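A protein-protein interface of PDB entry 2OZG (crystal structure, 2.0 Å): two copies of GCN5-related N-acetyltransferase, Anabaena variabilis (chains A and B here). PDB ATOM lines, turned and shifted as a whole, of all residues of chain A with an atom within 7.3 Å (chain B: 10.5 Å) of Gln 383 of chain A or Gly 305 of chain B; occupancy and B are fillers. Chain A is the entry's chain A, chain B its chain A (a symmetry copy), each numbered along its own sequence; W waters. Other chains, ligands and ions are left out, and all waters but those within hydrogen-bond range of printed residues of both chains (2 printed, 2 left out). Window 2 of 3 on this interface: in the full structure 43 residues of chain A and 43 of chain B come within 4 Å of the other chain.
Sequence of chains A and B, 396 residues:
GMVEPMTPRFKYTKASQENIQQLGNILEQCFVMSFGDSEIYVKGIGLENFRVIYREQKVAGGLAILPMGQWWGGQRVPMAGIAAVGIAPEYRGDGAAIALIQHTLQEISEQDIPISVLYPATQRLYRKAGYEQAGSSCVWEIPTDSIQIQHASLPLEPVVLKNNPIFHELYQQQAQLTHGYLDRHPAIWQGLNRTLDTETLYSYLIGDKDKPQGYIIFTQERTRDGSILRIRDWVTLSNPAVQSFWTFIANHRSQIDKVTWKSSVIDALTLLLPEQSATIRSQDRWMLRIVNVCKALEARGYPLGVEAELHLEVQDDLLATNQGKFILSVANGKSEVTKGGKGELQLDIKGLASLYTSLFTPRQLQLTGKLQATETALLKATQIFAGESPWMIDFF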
ATOM      1  N   TYR A 302     -14.493 -11.361   6.181  1.00  0.00           N
ATOM      2  CA  TYR A 302     -13.548 -11.951   7.114  1.00  0.00           C
ATOM      3  C   TYR A 302     -14.162 -13.185   7.727  1.00  0.00           C
ATOM      4  O   TYR A 302     -15.394 -13.300   7.813  1.00  0.00           O
ATOM      5  CB  TYR A 302     -13.165 -10.929   8.186  1.00  0.00           C
ATOM      6  CG  TYR A 302     -12.370  -9.788   7.578  1.00  0.00           C
ATOM      7  CD1 TYR A 302     -11.028  -9.913   7.376  1.00  0.00           C
ATOM      8  CD2 TYR A 302     -13.007  -8.661   7.061  1.00  0.00           C
ATOM      9  CE1 TYR A 302     -10.299  -8.913   6.757  1.00  0.00           C
ATOM     10  CE2 TYR A 302     -12.294  -7.673   6.411  1.00  0.00           C
ATOM     11  CZ  TYR A 302     -10.941  -7.795   6.283  1.00  0.00           C
ATOM     12  OH  TYR A 302     -10.180  -6.835   5.666  1.00  0.00           O
ATOM     13  N   PRO A 303     -13.320 -14.111   8.198  1.00  0.00           N
ATOM     14  CA  PRO A 303     -13.919 -15.306   8.782  1.00  0.00           C
ATOM     15  C   PRO A 303     -14.697 -15.001  10.039  1.00  0.00           C
ATOM     16  O   PRO A 303     -14.302 -14.145  10.818  1.00  0.00           O
ATOM     17  CB  PRO A 303     -12.704 -16.187   9.139  1.00  0.00           C
ATOM     18  CG  PRO A 303     -11.552 -15.615   8.438  1.00  0.00           C
ATOM     19  CD  PRO A 303     -11.856 -14.145   8.289  1.00  0.00           C
ATOM     20  N   LEU A 304     -15.810 -15.701  10.241  1.00  0.00           N
ATOM     21  CA  LEU A 304     -16.536 -15.599  11.487  1.00  0.00           C
ATOM     22  C   LEU A 304     -15.746 -16.299  12.615  1.00  0.00           C
ATOM     23  O   LEU A 304     -15.050 -17.296  12.395  1.00  0.00           O
ATOM     24  CB  LEU A 304     -17.927 -16.237  11.349  1.00  0.00           C
ATOM     25  CG  LEU A 304     -18.922 -15.552  10.410  1.00  0.00           C
ATOM     26  CD1 LEU A 304     -20.150 -16.446  10.219  1.00  0.00           C
ATOM     27  CD2 LEU A 304     -19.316 -14.166  10.996  1.00  0.00           C
ATOM     28  N   GLY A 305     -15.901 -15.774  13.810  1.00  0.00           N
ATOM     29  CA  GLY A 305     -15.273 -16.284  15.003  1.00  0.00           C
ATOM     30  C   GLY A 305     -13.995 -15.538  15.325  1.00  0.00           C
ATOM     31  O   GLY A 305     -13.378 -15.794  16.340  1.00  0.00           O
ATOM     32  N   VAL A 306     -13.590 -14.632  14.441  1.00  0.00           N
ATOM     33  CA  VAL A 306     -12.387 -13.852  14.636  1.00  0.00           C
ATOM     34  C   VAL A 306     -12.723 -12.481  15.245  1.00  0.00           C
ATOM     35  O   VAL A 306     -13.620 -11.764  14.787  1.00  0.00           O
ATOM     36  CB  VAL A 306     -11.629 -13.696  13.310  1.00  0.00           C
ATOM     37  CG1 VAL A 306     -10.430 -12.784  13.483  1.00  0.00           C
ATOM     38  CG2 VAL A 306     -11.213 -15.095  12.751  1.00  0.00           C
ATOM     39  N   GLU A 307     -12.043 -12.132  16.327  1.00  0.00           N
ATOM     40  CA  GLU A 307     -12.210 -10.799  16.889  1.00  0.00           C
ATOM     41  C   GLU A 307     -10.787 -10.336  17.158  1.00  0.00           C
ATOM     42  O   GLU A 307     -10.125 -10.842  18.079  1.00  0.00           O
ATOM     43  CB  GLU A 307     -13.094 -10.803  18.129  1.00  0.00           C
ATOM     44  CG  GLU A 307     -13.411  -9.407  18.637  1.00  0.00           C
ATOM     45  CD  GLU A 307     -14.406  -9.402  19.804  1.00  0.00           C
ATOM     46  OE1 GLU A 307     -15.195 -10.366  19.932  1.00  0.00           O
ATOM     47  OE2 GLU A 307     -14.392  -8.439  20.592  1.00  0.00           O
ATOM     48  N   ALA A 308     -10.308  -9.395  16.352  1.00  0.00           N
ATOM     49  CA  ALA A 308      -8.934  -8.947  16.482  1.00  0.00           C
ATOM     50  C   ALA A 308      -8.726  -7.586  15.920  1.00  0.00           C
ATOM     51  O   ALA A 308      -9.404  -7.184  14.984  1.00  0.00           O
ATOM     52  CB  ALA A 308      -8.017  -9.889  15.769  1.00  0.00           C
ATOM     53  N   VAL A 330     -11.360  -6.315  13.287  1.00  0.00           N
ATOM     54  CA  VAL A 330     -12.264  -7.334  12.718  1.00  0.00           C
ATOM     55  C   VAL A 330     -13.149  -7.981  13.797  1.00  0.00           C
ATOM     56  O   VAL A 330     -12.697  -8.356  14.887  1.00  0.00           O
ATOM     57  CB  VAL A 330     -11.446  -8.418  11.926  1.00  0.00           C
ATOM     58  CG1 VAL A 330     -12.357  -9.479  11.323  1.00  0.00           C
ATOM     59  CG2 VAL A 330     -10.639  -7.766  10.794  1.00  0.00           C
ATOM     60  N   PRO A 362       0.744 -15.153   6.714  1.00  0.00           N
ATOM     61  CA  PRO A 362       1.685 -14.244   7.315  1.00  0.00           C
ATOM     62  C   PRO A 362       3.046 -14.822   7.569  1.00  0.00           C
ATOM     63  O   PRO A 362       4.044 -14.156   7.293  1.00  0.00           O
ATOM     64  CB  PRO A 362       0.954 -13.783   8.619  1.00  0.00           C
ATOM     65  CG  PRO A 362      -0.454 -13.773   8.239  1.00  0.00           C
ATOM     66  CD  PRO A 362      -0.614 -15.010   7.297  1.00  0.00           C
ATOM     67  N   THR A 376       2.443 -11.761  18.149  1.00  0.00           N
ATOM     68  CA  THR A 376       1.036 -11.516  18.379  1.00  0.00           C
ATOM     69  C   THR A 376       0.385 -10.967  17.129  1.00  0.00           C
ATOM     70  O   THR A 376      -0.670 -11.448  16.695  1.00  0.00           O
ATOM     71  CB  THR A 376       0.845 -10.557  19.557  1.00  0.00           C
ATOM     72  OG1 THR A 376       1.546 -11.100  20.675  1.00  0.00           O
ATOM     73  CG2 THR A 376      -0.633 -10.464  19.896  1.00  0.00           C
ATOM     74  N   ALA A 377       1.030  -9.998  16.504  1.00  0.00           N
ATOM     75  CA  ALA A 377       0.487  -9.486  15.266  1.00  0.00           C
ATOM     76  C   ALA A 377       0.478 -10.592  14.209  1.00  0.00           C
ATOM     77  O   ALA A 377      -0.461 -10.689  13.449  1.00  0.00           O
ATOM     78  CB  ALA A 377       1.273  -8.326  14.789  1.00  0.00           C
ATOM     79  N   LEU A 378       1.488 -11.442  14.153  1.00  0.00           N
ATOM     80  CA  LEU A 378       1.483 -12.541  13.175  1.00  0.00           C
ATOM     81  C   LEU A 378       0.266 -13.421  13.385  1.00  0.00           C
ATOM     82  O   LEU A 378      -0.368 -13.838  12.438  1.00  0.00           O
ATOM     83  CB  LEU A 378       2.742 -13.405  13.260  1.00  0.00           C
ATOM     84  CG  LEU A 378       4.092 -12.917  12.717  1.00  0.00           C
ATOM     85  CD1 LEU A 378       5.102 -14.017  12.902  1.00  0.00           C
ATOM     86  CD2 LEU A 378       4.013 -12.547  11.235  1.00  0.00           C
ATOM     87  N   LEU A 379      -0.052 -13.709  14.654  1.00  0.00           N
ATOM     88  CA  LEU A 379      -1.203 -14.546  14.967  1.00  0.00           C
ATOM     89  C   LEU A 379      -2.509 -13.868  14.569  1.00  0.00           C
ATOM     90  O   LEU A 379      -3.378 -14.480  13.963  1.00  0.00           O
ATOM     91  CB  LEU A 379      -1.230 -14.938  16.451  1.00  0.00           C
ATOM     92  CG  LEU A 379      -2.466 -15.762  16.848  1.00  0.00           C
ATOM     93  CD1 LEU A 379      -2.548 -17.025  16.019  1.00  0.00           C
ATOM     94  CD2 LEU A 379      -2.477 -16.071  18.338  1.00  0.00           C
ATOM     95  N   LYS A 380      -2.658 -12.601  14.930  1.00  0.00           N
ATOM     96  CA  LYS A 380      -3.856 -11.868  14.576  1.00  0.00           C
ATOM     97  C   LYS A 380      -4.027 -11.836  13.053  1.00  0.00           C
ATOM     98  O   LYS A 380      -5.100 -12.169  12.542  1.00  0.00           O
ATOM     99  CB  LYS A 380      -3.827 -10.475  15.203  1.00  0.00           C
ATOM    100  CG  LYS A 380      -3.851 -10.532  16.681  1.00  0.00           C
ATOM    101  CD  LYS A 380      -4.023  -9.158  17.335  1.00  0.00           C
ATOM    102  CE  LYS A 380      -2.864  -8.174  16.997  1.00  0.00           C
ATOM    103  NZ  LYS A 380      -2.857  -7.008  17.954  1.00  0.00           N
ATOM    104  N   ALA A 381      -2.968 -11.518  12.323  1.00  0.00           N
ATOM    105  CA  ALA A 381      -3.054 -11.524  10.859  1.00  0.00           C
ATOM    106  C   ALA A 381      -3.368 -12.901  10.269  1.00  0.00           C
ATOM    107  O   ALA A 381      -4.049 -12.999   9.261  1.00  0.00           O
ATOM    108  CB  ALA A 381      -1.815 -11.031  10.264  1.00  0.00           C
ATOM    109  N   THR A 382      -2.870 -13.955  10.889  1.00  0.00           N
ATOM    110  CA  THR A 382      -3.158 -15.289  10.398  1.00  0.00           C
ATOM    111  C   THR A 382      -4.635 -15.583  10.552  1.00  0.00           C
ATOM    112  O   THR A 382      -5.251 -16.119   9.648  1.00  0.00           O
ATOM    113  CB  THR A 382      -2.329 -16.334  11.162  1.00  0.00           C
ATOM    114  OG1 THR A 382      -0.957 -16.033  10.994  1.00  0.00           O
ATOM    115  CG2 THR A 382      -2.579 -17.720  10.678  1.00  0.00           C
ATOM    116  N   GLN A 383      -5.194 -15.205  11.695  1.00  0.00           N
ATOM    117  CA  GLN A 383      -6.599 -15.439  11.968  1.00  0.00           C
ATOM    118  C   GLN A 383      -7.485 -14.627  11.008  1.00  0.00           C
ATOM    119  O   GLN A 383      -8.464 -15.150  10.443  1.00  0.00           O
ATOM    120  CB  GLN A 383      -6.913 -15.029  13.419  1.00  0.00           C
ATOM    121  CG  GLN A 383      -6.224 -15.922  14.477  1.00  0.00           C
ATOM    122  CD  GLN A 383      -6.335 -15.370  15.876  1.00  0.00           C
ATOM    123  OE1 GLN A 383      -6.563 -14.170  16.052  1.00  0.00           O
ATOM    124  NE2 GLN A 383      -6.127 -16.220  16.881  1.00  0.00           N
ATOM    125  N   ILE A 384      -7.126 -13.355  10.824  1.00  0.00           N
ATOM    126  CA  ILE A 384      -7.890 -12.427   9.948  1.00  0.00           C
ATOM    127  C   ILE A 384      -7.930 -12.834   8.482  1.00  0.00           C
ATOM    128  O   ILE A 384      -9.005 -12.803   7.833  1.00  0.00           O
ATOM    129  CB  ILE A 384      -7.322 -10.981  10.067  1.00  0.00           C
ATOM    130  CG1 ILE A 384      -7.581 -10.429  11.466  1.00  0.00           C
ATOM    131  CG2 ILE A 384      -7.928  -9.998   9.062  1.00  0.00           C
ATOM    132  CD1 ILE A 384      -6.843  -9.142  11.796  1.00  0.00           C
ATOM    133  N   PHE A 385      -6.763 -13.179   7.941  1.00  0.00           N
ATOM    134  CA  PHE A 385      -6.659 -13.381   6.480  1.00  0.00           C
ATOM    135  C   PHE A 385      -6.721 -14.810   5.995  1.00  0.00           C
ATOM    136  O   PHE A 385      -6.589 -15.039   4.810  1.00  0.00           O
ATOM    137  CB  PHE A 385      -5.394 -12.693   5.927  1.00  0.00           C
ATOM    138  CG  PHE A 385      -5.434 -11.184   6.072  1.00  0.00           C
ATOM    139  CD1 PHE A 385      -6.220 -10.414   5.199  1.00  0.00           C
ATOM    140  CD2 PHE A 385      -4.679 -10.545   7.043  1.00  0.00           C
ATOM    141  CE1 PHE A 385      -6.307  -9.031   5.359  1.00  0.00           C
ATOM    142  CE2 PHE A 385      -4.759  -9.135   7.221  1.00  0.00           C
ATOM    143  CZ  PHE A 385      -5.566  -8.400   6.370  1.00  0.00           C
ATOM    144  N   ALA A 386      -6.978 -15.745   6.896  1.00  0.00           N
ATOM    145  CA  ALA A 386      -7.032 -17.186   6.564  1.00  0.00           C
ATOM    146  C   ALA A 386      -8.165 -17.415   5.596  1.00  0.00           C
ATOM    147  O   ALA A 386      -9.196 -16.756   5.687  1.00  0.00           O
ATOM    148  CB  ALA A 386      -7.260 -18.002   7.826  1.00  0.00           C
ATOM    149  N   GLY A 387      -7.975 -18.344   4.670  1.00  0.00           N
ATOM    150  CA  GLY A 387      -8.988 -18.597   3.688  1.00  0.00           C
ATOM    151  C   GLY A 387      -8.531 -19.585   2.636  1.00  0.00           C
ATOM    152  O   GLY A 387      -7.373 -19.968   2.585  1.00  0.00           O
ATOM    153  N   GLY B 301      -2.192 -30.369  16.704  1.00  0.00           N
ATOM    154  CA  GLY B 301      -2.321 -28.985  17.141  1.00  0.00           C
ATOM    155  C   GLY B 301      -3.509 -28.324  16.454  1.00  0.00           C
ATOM    156  O   GLY B 301      -3.870 -28.703  15.328  1.00  0.00           O
ATOM    157  N   TYR B 302      -4.084 -27.306  17.106  1.00  0.00           N
ATOM    158  CA  TYR B 302      -5.212 -26.566  16.566  1.00  0.00           C
ATOM    159  C   TYR B 302      -4.891 -25.092  16.583  1.00  0.00           C
ATOM    160  O   TYR B 302      -4.079 -24.633  17.400  1.00  0.00           O
ATOM    161  CB  TYR B 302      -6.472 -26.869  17.380  1.00  0.00           C
ATOM    162  CG  TYR B 302      -6.896 -28.314  17.189  1.00  0.00           C
ATOM    163  CD1 TYR B 302      -7.641 -28.679  16.108  1.00  0.00           C
ATOM    164  CD2 TYR B 302      -6.403 -29.324  18.015  1.00  0.00           C
ATOM    165  CE1 TYR B 302      -7.976 -30.001  15.880  1.00  0.00           C
ATOM    166  CE2 TYR B 302      -6.702 -30.650  17.776  1.00  0.00           C
ATOM    167  CZ  TYR B 302      -7.506 -30.979  16.723  1.00  0.00           C
ATOM    168  OH  TYR B 302      -7.853 -32.277  16.452  1.00  0.00           O
ATOM    169  N   PRO B 303      -5.546 -24.319  15.709  1.00  0.00           N
ATOM    170  CA  PRO B 303      -5.225 -22.896  15.722  1.00  0.00           C
ATOM    171  C   PRO B 303      -5.633 -22.229  17.014  1.00  0.00           C
ATOM    172  O   PRO B 303      -6.658 -22.570  17.589  1.00  0.00           O
ATOM    173  CB  PRO B 303      -6.068 -22.320  14.567  1.00  0.00           C
ATOM    174  CG  PRO B 303      -6.523 -23.463  13.770  1.00  0.00           C
ATOM    175  CD  PRO B 303      -6.597 -24.623  14.732  1.00  0.00           C
ATOM    176  N   LEU B 304      -4.830 -21.276  17.477  1.00  0.00           N
ATOM    177  CA  LEU B 304      -5.213 -20.469  18.614  1.00  0.00           C
ATOM    178  C   LEU B 304      -6.340 -19.493  18.210  1.00  0.00           C
ATOM    179  O   LEU B 304      -6.405 -19.014  17.074  1.00  0.00           O
ATOM    180  CB  LEU B 304      -4.004 -19.682  19.143  1.00  0.00           C
ATOM    181  CG  LEU B 304      -2.862 -20.487  19.767  1.00  0.00           C
ATOM    182  CD1 LEU B 304      -1.661 -19.571  20.016  1.00  0.00           C
ATOM    183  CD2 LEU B 304      -3.355 -21.147  21.087  1.00  0.00           C
ATOM    184  N   GLY B 305      -7.187 -19.196  19.170  1.00  0.00           N
ATOM    185  CA  GLY B 305      -8.298 -18.291  19.014  1.00  0.00           C
ATOM    186  C   GLY B 305      -9.584 -19.030  18.709  1.00  0.00           C
ATOM    187  O   GLY B 305     -10.631 -18.421  18.620  1.00  0.00           O
ATOM    188  N   VAL B 306      -9.492 -20.343  18.526  1.00  0.00           N
ATOM    189  CA  VAL B 306     -10.649 -21.160  18.232  1.00  0.00           C
ATOM    190  C   VAL B 306     -11.194 -21.810  19.515  1.00  0.00           C
ATOM    191  O   VAL B 306     -10.456 -22.396  20.315  1.00  0.00           O
ATOM    192  CB  VAL B 306     -10.301 -22.223  17.180  1.00  0.00           C
ATOM    193  CG1 VAL B 306     -11.474 -23.157  16.953  1.00  0.00           C
ATOM    194  CG2 VAL B 306      -9.838 -21.544  15.851  1.00  0.00           C
ATOM    195  N   GLU B 307     -12.487 -21.656  19.753  1.00  0.00           N
ATOM    196  CA  GLU B 307     -13.105 -22.347  20.875  1.00  0.00           C
ATOM    197  C   GLU B 307     -14.380 -22.930  20.289  1.00  0.00           C
ATOM    198  O   GLU B 307     -15.329 -22.190  19.985  1.00  0.00           O
ATOM    199  CB  GLU B 307     -13.349 -21.419  22.059  1.00  0.00           C
ATOM    200  CG  GLU B 307     -13.843 -22.149  23.295  1.00  0.00           C
ATOM    201  CD  GLU B 307     -13.964 -21.240  24.525  1.00  0.00           C
ATOM    202  OE1 GLU B 307     -13.262 -20.205  24.585  1.00  0.00           O
ATOM    203  OE2 GLU B 307     -14.762 -21.560  25.424  1.00  0.00           O
ATOM    204  N   ALA B 308     -14.402 -24.247  20.110  1.00  0.00           N
ATOM    205  CA  ALA B 308     -15.544 -24.884  19.484  1.00  0.00           C
ATOM    206  C   ALA B 308     -15.657 -26.325  19.840  1.00  0.00           C
ATOM    207  O   ALA B 308     -14.659 -26.988  20.090  1.00  0.00           O
ATOM    208  CB  ALA B 308     -15.436 -24.782  17.995  1.00  0.00           C
ATOM    209  N   VAL B 330     -12.392 -28.112  21.119  1.00  0.00           N
ATOM    210  CA  VAL B 330     -11.121 -27.393  20.900  1.00  0.00           C
ATOM    211  C   VAL B 330     -11.087 -26.050  21.648  1.00  0.00           C
ATOM    212  O   VAL B 330     -12.041 -25.262  21.638  1.00  0.00           O
ATOM    213  CB  VAL B 330     -10.854 -27.198  19.363  1.00  0.00           C
ATOM    214  CG1 VAL B 330      -9.546 -26.463  19.109  1.00  0.00           C
ATOM    215  CG2 VAL B 330     -10.802 -28.554  18.646  1.00  0.00           C
ATOM    216  N   ALA B 331      -9.975 -25.791  22.317  1.00  0.00           N
ATOM    217  CA  ALA B 331      -9.771 -24.514  22.999  1.00  0.00           C
ATOM    218  C   ALA B 331      -8.285 -24.420  23.291  1.00  0.00           C
ATOM    219  O   ALA B 331      -7.609 -25.440  23.477  1.00  0.00           O
ATOM    220  CB  ALA B 331     -10.530 -24.445  24.244  1.00  0.00           C
ATOM    221  N   ASN B 332      -7.769 -23.201  23.222  1.00  0.00           N
ATOM    222  CA  ASN B 332      -6.386 -22.905  23.542  1.00  0.00           C
ATOM    223  C   ASN B 332      -5.417 -23.740  22.784  1.00  0.00           C
ATOM    224  O   ASN B 332      -4.365 -24.106  23.303  1.00  0.00           O
ATOM    225  CB  ASN B 332      -6.151 -23.096  25.037  1.00  0.00           C
ATOM    226  CG  ASN B 332      -7.127 -22.333  25.864  1.00  0.00           C
ATOM    227  OD1 ASN B 332      -7.954 -22.937  26.522  1.00  0.00           O
ATOM    228  ND2 ASN B 332      -7.109 -21.010  25.766  1.00  0.00           N
ATOM    229  N   GLY B 333      -5.751 -24.012  21.537  1.00  0.00           N
ATOM    230  CA  GLY B 333      -4.846 -24.774  20.644  1.00  0.00           C
ATOM    231  C   GLY B 333      -4.806 -26.277  20.866  1.00  0.00           C
ATOM    232  O   GLY B 333      -4.067 -26.995  20.182  1.00  0.00           O
ATOM    233  N   LYS B 334      -5.646 -26.759  21.756  1.00  0.00           N
ATOM    234  CA  LYS B 334      -5.676 -28.160  22.136  1.00  0.00           C
ATOM    235  C   LYS B 334      -7.091 -28.700  22.043  1.00  0.00           C
ATOM    236  O   LYS B 334      -8.026 -27.926  22.019  1.00  0.00           O
ATOM    237  CB  LYS B 334      -5.181 -28.292  23.554  1.00  0.00           C
ATOM    238  CG  LYS B 334      -3.888 -27.562  23.864  1.00  0.00           C
ATOM    239  CD  LYS B 334      -3.530 -27.737  25.341  1.00  0.00           C
ATOM    240  CE  LYS B 334      -3.836 -26.513  26.170  1.00  0.00           C
ATOM    241  NZ  LYS B 334      -2.651 -25.594  26.114  1.00  0.00           N
ATOM    242  N   LEU B 379     -19.111 -24.478   9.892  1.00  0.00           N
ATOM    243  CA  LEU B 379     -18.322 -23.345  10.355  1.00  0.00           C
ATOM    244  C   LEU B 379     -17.335 -23.761  11.441  1.00  0.00           C
ATOM    245  O   LEU B 379     -16.170 -23.392  11.408  1.00  0.00           O
ATOM    246  CB  LEU B 379     -19.214 -22.197  10.850  1.00  0.00           C
ATOM    247  CG  LEU B 379     -18.428 -21.005  11.419  1.00  0.00           C
ATOM    248  CD1 LEU B 379     -17.478 -20.455  10.379  1.00  0.00           C
ATOM    249  CD2 LEU B 379     -19.359 -19.925  11.951  1.00  0.00           C
ATOM    250  N   LYS B 380     -17.810 -24.516  12.422  1.00  0.00           N
ATOM    251  CA  LYS B 380     -16.943 -24.978  13.485  1.00  0.00           C
ATOM    252  C   LYS B 380     -15.794 -25.811  12.907  1.00  0.00           C
ATOM    253  O   LYS B 380     -14.626 -25.556  13.214  1.00  0.00           O
ATOM    254  CB  LYS B 380     -17.754 -25.730  14.539  1.00  0.00           C
ATOM    255  CG  LYS B 380     -18.733 -24.851  15.216  1.00  0.00           C
ATOM    256  CD  LYS B 380     -19.421 -25.521  16.408  1.00  0.00           C
ATOM    257  CE  LYS B 380     -20.236 -26.786  16.010  1.00  0.00           C
ATOM    258  NZ  LYS B 380     -21.199 -27.169  17.107  1.00  0.00           N
ATOM    259  N   THR B 382     -14.551 -25.658   9.915  1.00  0.00           N
ATOM    260  CA  THR B 382     -13.673 -24.809   9.135  1.00  0.00           C
ATOM    261  C   THR B 382     -12.694 -24.107  10.052  1.00  0.00           C
ATOM    262  O   THR B 382     -11.516 -24.031   9.750  1.00  0.00           O
ATOM    263  CB  THR B 382     -14.488 -23.775   8.342  1.00  0.00           C
ATOM    264  OG1 THR B 382     -15.386 -24.464   7.494  1.00  0.00           O
ATOM    265  CG2 THR B 382     -13.625 -22.891   7.510  1.00  0.00           C
ATOM    266  N   GLN B 383     -13.192 -23.619  11.182  1.00  0.00           N
ATOM    267  CA  GLN B 383     -12.359 -22.915  12.138  1.00  0.00           C
ATOM    268  C   GLN B 383     -11.311 -23.861  12.748  1.00  0.00           C
ATOM    269  O   GLN B 383     -10.121 -23.511  12.860  1.00  0.00           O
ATOM    270  CB  GLN B 383     -13.244 -22.343  13.262  1.00  0.00           C
ATOM    271  CG  GLN B 383     -14.204 -21.228  12.787  1.00  0.00           C
ATOM    272  CD  GLN B 383     -15.228 -20.851  13.827  1.00  0.00           C
ATOM    273  OE1 GLN B 383     -15.506 -21.636  14.737  1.00  0.00           O
ATOM    274  NE2 GLN B 383     -15.836 -19.672  13.680  1.00  0.00           N
ATOM    275  N   ILE B 384     -11.762 -25.057  13.129  1.00  0.00           N
ATOM    276  CA  ILE B 384     -10.883 -26.079  13.761  1.00  0.00           C
ATOM    277  C   ILE B 384      -9.748 -26.569  12.873  1.00  0.00           C
ATOM    278  O   ILE B 384      -8.580 -26.677  13.322  1.00  0.00           O
ATOM    279  CB  ILE B 384     -11.729 -27.297  14.238  1.00  0.00           C
ATOM    280  CG1 ILE B 384     -12.653 -26.881  15.379  1.00  0.00           C
ATOM    281  CG2 ILE B 384     -10.885 -28.475  14.732  1.00  0.00           C
ATOM    282  CD1 ILE B 384     -13.717 -27.900  15.751  1.00  0.00           C
ATOM    283  N   ALA B 386      -8.555 -25.415   9.850  1.00  0.00           N
ATOM    284  CA  ALA B 386      -7.916 -24.454   8.925  1.00  0.00           C
ATOM    285  C   ALA B 386      -6.422 -24.521   9.117  1.00  0.00           C
ATOM    286  O   ALA B 386      -5.953 -24.720  10.234  1.00  0.00           O
ATOM    287  CB  ALA B 386      -8.410 -23.047   9.215  1.00  0.00           C
ATOM    288  N   GLY B 387      -5.677 -24.359   8.033  1.00  0.00           N
ATOM    289  CA  GLY B 387      -4.249 -24.445   8.124  1.00  0.00           C
ATOM    290  C   GLY B 387      -3.584 -24.377   6.765  1.00  0.00           C
ATOM    291  O   GLY B 387      -4.239 -24.406   5.735  1.00  0.00           O
ATOM    292  N   GLU B 388      -2.278 -24.255   6.778  1.00  0.00           N
ATOM    293  CA  GLU B 388      -1.508 -24.201   5.567  1.00  0.00           C
ATOM    294  C   GLU B 388      -1.700 -25.551   4.842  1.00  0.00           C
ATOM    295  O   GLU B 388      -1.835 -26.603   5.485  1.00  0.00           O
ATOM    296  CB  GLU B 388      -0.030 -23.892   5.874  1.00  0.00           C
ATOM    297  CG  GLU B 388       0.210 -22.482   6.491  1.00  0.00           C
ATOM    298  CD  GLU B 388       1.698 -22.105   6.639  1.00  0.00           C
ATOM    299  OE1 GLU B 388       2.529 -22.931   6.208  1.00  0.00           O
ATOM    300  OE2 GLU B 388       2.023 -20.991   7.157  1.00  0.00           O
HETATM  301  O   HOH W   1     -10.062 -16.397  16.274  1.00  0.00           O
HETATM  302  O   HOH W   2     -12.691 -18.847  15.985  1.00  0.00           O
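The backbone carbonyl oxygen of Leu 304 of chain A is in hydrogen-bond range of the side-chain amide nitrogen of Gln 383 of chain B.
The backbone carbonyl oxygen of Leu 304 of chain B lies within hydrogen-bond range of the side-chain amide nitrogen of Gln 383 of chain A, 2.8 Å away.
Of the 21 printed residues of chain B, 4 touch a printed residue of chain A.
Hydrophobic or aromatic side chains of chain B within 4 Å of the printed part of chain A: Leu 304 and Leu 379.
Printed residues of chain A that touch a printed residue of chain B: Leu 304, Gly 305, Leu 379 and Gln 383.
Hydrophobic or aromatic side chains of chain A that line the printed part of chain B: Leu 304 and Leu 379.
Among the printed residues, merely in contact across the chains: Leu 304 of chain A with Leu 379 of chain B, Gly 305 of chain A with Gln 383 of chain B, Leu 379 of chain A with Leu 304 of chain B and Gln 383 of chain A with Gly 305 of chain B.
Leu 304 of chain A touches Gln 383 of chain B, and with the chains exchanged Gln 383 of chain A touches Leu 304 of chain B.
Gly 305 of chain A touches Gln 383 of chain B, and with the chains exchanged Gln 383 of chain A touches Gly 305 of chain B.
Of the 6 pairs that touch across the chains among the printed residues, 6 have their exchanged pair printed and touching as well.
Of the printed residues of chain B, Gly 305 of chain A touches Gln 383 (3.7 Å).
Val 330 of chain A touches none of the printed residues of chain B.
Lys 380 of chain A touches none of the printed residues of chain B.
No residue of chain B comes within 4 Å of Ala 381 of chain A.
No residue of chain B comes within 4 Å of Thr 382 of chain A.
Gln 383 of chain A touches just these residues of chain B: Leu 304 and Gly 305.
No residue of chain B comes within 4 Å of Ile 384 of chain A.
No residue of chain B comes within 4 Å of Ala 386 of chain A.
Of the printed residues of chain A, Leu 304 of chain B touches Leu 379 (3.97 Å) and Gln 383 (2.8 Å).
Of the printed residues of chain A, Leu 379 of chain B touches Leu 304.
Of the printed residues of chain A, Gln 383 of chain B touches Leu 304 and Gly 305.
The nearest residue of chain B that does not touch Gln 383 of chain A is Val 306 of chain B (5.6 Å).
The nearest residue of chain A that does not touch Gly 305 of chain B is Gly 305 of chain A (4.4 Å).
The nearest printed residue of chain A that does not touch Leu 304 of chain B is Val 306 of chain A (7.6 Å).
Water W1 bridges O of Gly 305 of chain B (3.2 Å) and O of Gly 305 of chain A (3.4 Å).
Water W2 lies within hydrogen-bond range of the backbone carbonyl oxygen (O) of Gly 305 of chain A and the backbone carbonyl oxygen (O) of Gly 305 of chain B.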
